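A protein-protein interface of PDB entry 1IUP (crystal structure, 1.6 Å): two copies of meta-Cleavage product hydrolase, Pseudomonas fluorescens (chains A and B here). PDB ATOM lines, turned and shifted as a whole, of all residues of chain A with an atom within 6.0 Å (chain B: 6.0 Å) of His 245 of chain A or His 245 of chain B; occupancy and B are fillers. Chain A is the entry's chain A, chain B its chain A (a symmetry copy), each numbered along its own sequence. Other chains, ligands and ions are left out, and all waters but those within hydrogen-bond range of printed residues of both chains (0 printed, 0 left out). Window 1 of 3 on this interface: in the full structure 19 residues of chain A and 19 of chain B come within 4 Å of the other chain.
The backbone NH (N) of His 245 of chain A is in hydrogen-bond range of the backbone carbonyl oxygen (O) of Ile 218 of chain A (2.7 Å). N of His 220 of chain B sits at hydrogen-bond distance from O of His 245 of chain B. N of His 220 of chain A lies within hydrogen-bond range of O of His 245 of chain A. N of Ile 218 of chain B is in hydrogen-bond range of O of Gln 243 of chain B. O of Ile 218 of chain B sits at hydrogen-bond distance from N of His 245 of chain B, at 2.7 Å. O of Gln 243 of chain A is in hydrogen-bond range of N of Ile 218 of chain A, at 2.8 Å.
The backbone carbonyl oxygen (O) of Leu 244 of chain B lies close to the backbone carbonyl oxygen (O) of Leu 244 of chain A, 3.4 Å away. A ring nitrogen (NE2) of His 245 of chain B is in hydrogen-bond range of the side-chain amide oxygen (OE1) of Gln 243 of chain A (2.8 Å). A ring nitrogen (ND1) of His 245 of chain B sits at hydrogen-bond distance from a ring nitrogen (ND1) of His 245 of chain A (2.7 Å). A ring nitrogen (NE2) of His 245 of chain A lies within hydrogen-bond range of the side-chain amide oxygen of Gln 243 of chain B (2.8 Å). The backbone NH of Val 246 of chain B lies within hydrogen-bond range of the backbone carbonyl oxygen of Leu 244 of chain A. The backbone NH of Val 246 of chain A is in hydrogen-bond range of the backbone carbonyl oxygen of Leu 244 of chain B.
Among the printed residues, merely in contact across the chains: Leu 244 of chain A with His 245 of chain B, His 245 of chain A with Leu 244 of chain B, Val 246 of chain A with Gln 243 of chain B, Gln 243 of chain A with Val 246 of chain B, Gln 243 of chain A with Phe 247 of chain B, Phe 247 of chain A with Gln 243 of chain B and Leu 265 of chain A with Leu 265 of chain B.
His 245 of chain A touches just these residues of chain B: Gln 243 (2.8 Å), Leu 244 (3.1 Å) and His 245 (2.7 Å). Of chain A, only Gln 243, Leu 244 and His 245 come within 4 Å of His 245 of chain B. Printed residues of chain A within 4 Å of Leu 265 of chain B: Leu 265. Printed residues of chain B within 4 Å of Val 246 of chain A: Gln 243 and Leu 244. Of the printed residues of chain A, Phe 247 of chain B touches Gln 243. Of the printed residues of chain B, Leu 265 of chain A touches Leu 265 (3.6 Å). Ile 218 of chain A touches none of the printed residues of chain B. Ile 218 of chain B touches none of the printed residues of chain A. The nearest residue of chain B that does not touch His 245 of chain A is Leu 217 of chain B (4.4 Å). The nearest printed residue of chain B that does not touch Val 246 of chain A is His 245 of chain B (5.0 Å).
Of the 11 printed residues of chain A, 6 touch a printed residue of chain B. Hydrophobic or aromatic side chains of chain A within 4 Å of the printed part of chain B: His 245, Phe 247 and Leu 265. Hydrophobic or aromatic side chains of chain B within 4 Å of the printed part of chain A: His 245, Phe 247 and Leu 265. Among the printed residues, 13 pairs touch across the chains. Among the printed residues, no Asp or Glu carboxylate lies within 4 Å of a Lys or Arg side-chain nitrogen of the other chain.
Gln 243 of chain A touches Phe 247 of chain B, and with the chains exchanged Phe 247 of chain A touches Gln 243 of chain B. Leu 244 of chain A touches its own counterpart, Leu 244 of chain B. Leu 244 of chain A touches Val 246 of chain B, and with the chains exchanged Val 246 of chain A touches Leu 244 of chain B. His 245 of chain B touches its own counterpart, His 245 of chain A. Positions printed for both chains: 217, 218, 219, 220, 221, 243, 244, 245, 246, 247 and 265.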
ATOM      1  N   LEU A 217      26.625  38.176   6.954  1.00  0.00           N
ATOM      2  CA  LEU A 217      26.136  36.808   6.856  1.00  0.00           C
ATOM      3  C   LEU A 217      27.350  35.925   6.583  1.00  0.00           C
ATOM      4  O   LEU A 217      27.984  36.039   5.534  1.00  0.00           O
ATOM      5  CB  LEU A 217      25.117  36.680   5.720  1.00  0.00           C
ATOM      6  CG  LEU A 217      24.615  35.269   5.389  1.00  0.00           C
ATOM      7  CD1 LEU A 217      23.985  34.622   6.619  1.00  0.00           C
ATOM      8  CD2 LEU A 217      23.608  35.360   4.247  1.00  0.00           C
ATOM      9  N   ILE A 218      27.672  35.058   7.539  1.00  0.00           N
ATOM     10  CA  ILE A 218      28.816  34.159   7.430  1.00  0.00           C
ATOM     11  C   ILE A 218      28.310  32.778   7.015  1.00  0.00           C
ATOM     12  O   ILE A 218      27.464  32.194   7.687  1.00  0.00           O
ATOM     13  CB  ILE A 218      29.544  34.059   8.782  1.00  0.00           C
ATOM     14  CG1 ILE A 218      29.847  35.469   9.308  1.00  0.00           C
ATOM     15  CG2 ILE A 218      30.833  33.265   8.626  1.00  0.00           C
ATOM     16  CD1 ILE A 218      30.328  35.491  10.751  1.00  0.00           C
ATOM     17  N   ILE A 219      28.830  32.269   5.901  1.00  0.00           N
ATOM     18  CA  ILE A 219      28.416  30.974   5.368  1.00  0.00           C
ATOM     19  C   ILE A 219      29.604  30.023   5.280  1.00  0.00           C
ATOM     20  O   ILE A 219      30.690  30.423   4.866  1.00  0.00           O
ATOM     21  CB  ILE A 219      27.803  31.153   3.961  1.00  0.00           C
ATOM     22  CG1 ILE A 219      26.555  32.033   4.063  1.00  0.00           C
ATOM     23  CG2 ILE A 219      27.486  29.793   3.339  1.00  0.00           C
ATOM     24  CD1 ILE A 219      25.926  32.380   2.734  1.00  0.00           C
ATOM     25  N   HIS A 220      29.396  28.764   5.657  1.00  0.00           N
ATOM     26  CA  HIS A 220      30.479  27.786   5.617  1.00  0.00           C
ATOM     27  C   HIS A 220      29.938  26.376   5.399  1.00  0.00           C
ATOM     28  O   HIS A 220      28.831  26.050   5.829  1.00  0.00           O
ATOM     29  CB  HIS A 220      31.267  27.825   6.937  1.00  0.00           C
ATOM     30  CG  HIS A 220      32.728  27.521   6.787  1.00  0.00           C
ATOM     31  ND1 HIS A 220      33.695  28.503   6.808  1.00  0.00           N
ATOM     32  CD2 HIS A 220      33.386  26.352   6.592  1.00  0.00           C
ATOM     33  CE1 HIS A 220      34.884  27.954   6.630  1.00  0.00           C
ATOM     34  NE2 HIS A 220      34.724  26.649   6.496  1.00  0.00           N
ATOM     35  N   GLY A 221      30.723  25.551   4.716  1.00  0.00           N
ATOM     36  CA  GLY A 221      30.334  24.169   4.492  1.00  0.00           C
ATOM     37  C   GLY A 221      30.957  23.361   5.617  1.00  0.00           C
ATOM     38  O   GLY A 221      32.155  23.467   5.866  1.00  0.00           O
ATOM     39  N   GLN A 243      25.280  36.709  11.378  1.00  0.00           N
ATOM     40  CA  GLN A 243      24.472  35.504  11.331  1.00  0.00           C
ATOM     41  C   GLN A 243      25.425  34.475  10.754  1.00  0.00           C
ATOM     42  O   GLN A 243      26.251  34.798   9.895  1.00  0.00           O
ATOM     43  CB  GLN A 243      23.279  35.646  10.387  1.00  0.00           C
ATOM     44  CG  GLN A 243      22.182  36.565  10.869  1.00  0.00           C
ATOM     45  CD  GLN A 243      21.064  36.666   9.860  1.00  0.00           C
ATOM     46  OE1 GLN A 243      20.227  35.765   9.741  1.00  0.00           O
ATOM     47  NE2 GLN A 243      21.052  37.760   9.107  1.00  0.00           N
ATOM     48  N   LEU A 244      25.324  33.245  11.232  1.00  0.00           N
ATOM     49  CA  LEU A 244      26.173  32.175  10.741  1.00  0.00           C
ATOM     50  C   LEU A 244      25.283  31.097  10.160  1.00  0.00           C
ATOM     51  O   LEU A 244      24.312  30.685  10.791  1.00  0.00           O
ATOM     52  CB  LEU A 244      26.996  31.581  11.885  1.00  0.00           C
ATOM     53  CG  LEU A 244      27.811  30.324  11.564  1.00  0.00           C
ATOM     54  CD1 LEU A 244      28.921  30.657  10.579  1.00  0.00           C
ATOM     55  CD2 LEU A 244      28.396  29.759  12.850  1.00  0.00           C
ATOM     56  N   HIS A 245      25.592  30.658   8.948  1.00  0.00           N
ATOM     57  CA  HIS A 245      24.815  29.596   8.345  1.00  0.00           C
ATOM     58  C   HIS A 245      25.789  28.529   7.864  1.00  0.00           C
ATOM     59  O   HIS A 245      26.620  28.777   6.987  1.00  0.00           O
ATOM     60  CB  HIS A 245      23.982  30.101   7.169  1.00  0.00           C
ATOM     61  CG  HIS A 245      22.915  29.140   6.754  1.00  0.00           C
ATOM     62  ND1 HIS A 245      21.641  29.174   7.279  1.00  0.00           N
ATOM     63  CD2 HIS A 245      22.956  28.063   5.935  1.00  0.00           C
ATOM     64  CE1 HIS A 245      20.945  28.155   6.804  1.00  0.00           C
ATOM     65  NE2 HIS A 245      21.720  27.465   5.986  1.00  0.00           N
ATOM     66  N   VAL A 246      25.695  27.348   8.465  1.00  0.00           N
ATOM     67  CA  VAL A 246      26.567  26.237   8.115  1.00  0.00           C
ATOM     68  C   VAL A 246      25.776  25.170   7.376  1.00  0.00           C
ATOM     69  O   VAL A 246      24.753  24.699   7.864  1.00  0.00           O
ATOM     70  CB  VAL A 246      27.190  25.589   9.375  1.00  0.00           C
ATOM     71  CG1 VAL A 246      28.096  24.427   8.969  1.00  0.00           C
ATOM     72  CG2 VAL A 246      27.981  26.626  10.158  1.00  0.00           C
ATOM     73  N   PHE A 247      26.255  24.801   6.193  1.00  0.00           N
ATOM     74  CA  PHE A 247      25.604  23.772   5.391  1.00  0.00           C
ATOM     75  C   PHE A 247      26.265  22.423   5.627  1.00  0.00           C
ATOM     76  O   PHE A 247      27.469  22.276   5.407  1.00  0.00           O
ATOM     77  CB  PHE A 247      25.734  24.069   3.891  1.00  0.00           C
ATOM     78  CG  PHE A 247      24.963  25.267   3.420  1.00  0.00           C
ATOM     79  CD1 PHE A 247      23.570  25.279   3.449  1.00  0.00           C
ATOM     80  CD2 PHE A 247      25.632  26.360   2.882  1.00  0.00           C
ATOM     81  CE1 PHE A 247      22.856  26.366   2.944  1.00  0.00           C
ATOM     82  CE2 PHE A 247      24.929  27.450   2.374  1.00  0.00           C
ATOM     83  CZ  PHE A 247      23.539  27.455   2.403  1.00  0.00           C
ATOM     84  N   LEU A 265      19.422  32.650   0.477  1.00  0.00           N
ATOM     85  CA  LEU A 265      19.879  33.284   1.709  1.00  0.00           C
ATOM     86  C   LEU A 265      20.467  34.659   1.434  1.00  0.00           C
ATOM     87  O   LEU A 265      20.166  35.625   2.135  1.00  0.00           O
ATOM     88  CB  LEU A 265      20.940  32.419   2.393  1.00  0.00           C
ATOM     89  CG  LEU A 265      20.462  31.216   3.202  1.00  0.00           C
ATOM     90  CD1 LEU A 265      21.660  30.364   3.600  1.00  0.00           C
ATOM     91  CD2 LEU A 265      19.710  31.704   4.439  1.00  0.00           C
ATOM     92  N   LEU B 217      16.924  21.683  10.275  1.00  0.00           N
ATOM     93  CA  LEU B 217      17.399  23.057  10.361  1.00  0.00           C
ATOM     94  C   LEU B 217      17.560  23.374  11.845  1.00  0.00           C
ATOM     95  O   LEU B 217      16.581  23.402  12.589  1.00  0.00           O
ATOM     96  CB  LEU B 217      16.395  24.016   9.716  1.00  0.00           C
ATOM     97  CG  LEU B 217      16.677  25.517   9.854  1.00  0.00           C
ATOM     98  CD1 LEU B 217      18.046  25.861   9.275  1.00  0.00           C
ATOM     99  CD2 LEU B 217      15.575  26.293   9.140  1.00  0.00           C
ATOM    100  N   ILE B 218      18.802  23.598  12.264  1.00  0.00           N
ATOM    101  CA  ILE B 218      19.117  23.898  13.658  1.00  0.00           C
ATOM    102  C   ILE B 218      19.310  25.408  13.798  1.00  0.00           C
ATOM    103  O   ILE B 218      20.141  25.997  13.113  1.00  0.00           O
ATOM    104  CB  ILE B 218      20.405  23.169  14.080  1.00  0.00           C
ATOM    105  CG1 ILE B 218      20.293  21.680  13.723  1.00  0.00           C
ATOM    106  CG2 ILE B 218      20.637  23.338  15.575  1.00  0.00           C
ATOM    107  CD1 ILE B 218      21.606  20.922  13.858  1.00  0.00           C
ATOM    108  N   ILE B 219      18.532  26.023  14.684  1.00  0.00           N
ATOM    109  CA  ILE B 219      18.585  27.466  14.899  1.00  0.00           C
ATOM    110  C   ILE B 219      18.941  27.782  16.347  1.00  0.00           C
ATOM    111  O   ILE B 219      18.429  27.147  17.266  1.00  0.00           O
ATOM    112  CB  ILE B 219      17.217  28.101  14.563  1.00  0.00           C
ATOM    113  CG1 ILE B 219      16.900  27.864  13.084  1.00  0.00           C
ATOM    114  CG2 ILE B 219      17.219  29.591  14.908  1.00  0.00           C
ATOM    115  CD1 ILE B 219      15.532  28.338  12.655  1.00  0.00           C
ATOM    116  N   HIS B 220      19.809  28.770  16.551  1.00  0.00           N
ATOM    117  CA  HIS B 220      20.218  29.135  17.904  1.00  0.00           C
ATOM    118  C   HIS B 220      20.602  30.610  17.983  1.00  0.00           C
ATOM    119  O   HIS B 220      21.096  31.187  17.014  1.00  0.00           O
ATOM    120  CB  HIS B 220      21.420  28.278  18.336  1.00  0.00           C
ATOM    121  CG  HIS B 220      21.455  27.967  19.803  1.00  0.00           C
ATOM    122  ND1 HIS B 220      21.086  26.739  20.308  1.00  0.00           N
ATOM    123  CD2 HIS B 220      21.792  28.727  20.873  1.00  0.00           C
ATOM    124  CE1 HIS B 220      21.193  26.756  21.626  1.00  0.00           C
ATOM    125  NE2 HIS B 220      21.618  27.951  21.994  1.00  0.00           N
ATOM    126  N   GLY B 221      20.354  31.214  19.140  1.00  0.00           N
ATOM    127  CA  GLY B 221      20.724  32.603  19.348  1.00  0.00           C
ATOM    128  C   GLY B 221      22.103  32.589  19.984  1.00  0.00           C
ATOM    129  O   GLY B 221      22.319  31.902  20.980  1.00  0.00           O
ATOM    130  N   GLN B 243      21.512  21.817   8.706  1.00  0.00           N
ATOM    131  CA  GLN B 243      21.955  23.172   8.432  1.00  0.00           C
ATOM    132  C   GLN B 243      21.895  23.834   9.795  1.00  0.00           C
ATOM    133  O   GLN B 243      21.005  23.537  10.597  1.00  0.00           O
ATOM    134  CB  GLN B 243      21.006  23.911   7.490  1.00  0.00           C
ATOM    135  CG  GLN B 243      21.022  23.436   6.057  1.00  0.00           C
ATOM    136  CD  GLN B 243      20.033  24.200   5.211  1.00  0.00           C
ATOM    137  OE1 GLN B 243      20.282  25.343   4.812  1.00  0.00           O
ATOM    138  NE2 GLN B 243      18.888  23.583   4.945  1.00  0.00           N
ATOM    139  N   LEU B 244      22.846  24.715  10.064  1.00  0.00           N
ATOM    140  CA  LEU B 244      22.878  25.422  11.332  1.00  0.00           C
ATOM    141  C   LEU B 244      22.782  26.906  11.044  1.00  0.00           C
ATOM    142  O   LEU B 244      23.499  27.422  10.190  1.00  0.00           O
ATOM    143  CB  LEU B 244      24.189  25.139  12.065  1.00  0.00           C
ATOM    144  CG  LEU B 244      24.454  25.952  13.337  1.00  0.00           C
ATOM    145  CD1 LEU B 244      23.453  25.574  14.418  1.00  0.00           C
ATOM    146  CD2 LEU B 244      25.874  25.693  13.817  1.00  0.00           C
ATOM    147  N   HIS B 245      21.878  27.588  11.734  1.00  0.00           N
ATOM    148  CA  HIS B 245      21.760  29.020  11.547  1.00  0.00           C
ATOM    149  C   HIS B 245      21.803  29.667  12.924  1.00  0.00           C
ATOM    150  O   HIS B 245      20.928  29.438  13.762  1.00  0.00           O
ATOM    151  CB  HIS B 245      20.457  29.392  10.843  1.00  0.00           C
ATOM    152  CG  HIS B 245      20.456  30.792  10.319  1.00  0.00           C
ATOM    153  ND1 HIS B 245      20.881  31.107   9.046  1.00  0.00           N
ATOM    154  CD2 HIS B 245      20.171  31.969  10.923  1.00  0.00           C
ATOM    155  CE1 HIS B 245      20.861  32.420   8.891  1.00  0.00           C
ATOM    156  NE2 HIS B 245      20.434  32.967  10.016  1.00  0.00           N
ATOM    157  N   VAL B 246      22.845  30.460  13.157  1.00  0.00           N
ATOM    158  CA  VAL B 246      23.023  31.139  14.431  1.00  0.00           C
ATOM    159  C   VAL B 246      22.781  32.631  14.262  1.00  0.00           C
ATOM    160  O   VAL B 246      23.393  33.270  13.412  1.00  0.00           O
ATOM    161  CB  VAL B 246      24.455  30.942  14.981  1.00  0.00           C
ATOM    162  CG1 VAL B 246      24.605  31.670  16.316  1.00  0.00           C
ATOM    163  CG2 VAL B 246      24.749  29.459  15.153  1.00  0.00           C
ATOM    164  N   PHE B 247      21.880  33.173  15.073  1.00  0.00           N
ATOM    165  CA  PHE B 247      21.570  34.597  15.029  1.00  0.00           C
ATOM    166  C   PHE B 247      22.373  35.344  16.082  1.00  0.00           C
ATOM    167  O   PHE B 247      22.271  35.038  17.272  1.00  0.00           O
ATOM    168  CB  PHE B 247      20.090  34.854  15.340  1.00  0.00           C
ATOM    169  CG  PHE B 247      19.134  34.367  14.292  1.00  0.00           C
ATOM    170  CD1 PHE B 247      19.115  34.934  13.020  1.00  0.00           C
ATOM    171  CD2 PHE B 247      18.204  33.381  14.599  1.00  0.00           C
ATOM    172  CE1 PHE B 247      18.177  34.527  12.070  1.00  0.00           C
ATOM    173  CE2 PHE B 247      17.262  32.967  13.661  1.00  0.00           C
ATOM    174  CZ  PHE B 247      17.247  33.540  12.394  1.00  0.00           C
ATOM    175  N   LEU B 265      13.185  31.706   7.122  1.00  0.00           N
ATOM    176  CA  LEU B 265      14.047  30.530   7.050  1.00  0.00           C
ATOM    177  C   LEU B 265      13.232  29.248   7.126  1.00  0.00           C
ATOM    178  O   LEU B 265      13.450  28.317   6.352  1.00  0.00           O
ATOM    179  CB  LEU B 265      15.062  30.542   8.193  1.00  0.00           C
ATOM    180  CG  LEU B 265      16.290  31.437   8.045  1.00  0.00           C
ATOM    181  CD1 LEU B 265      17.046  31.485   9.366  1.00  0.00           C
ATOM    182  CD2 LEU B 265      17.182  30.890   6.931  1.00  0.00           C
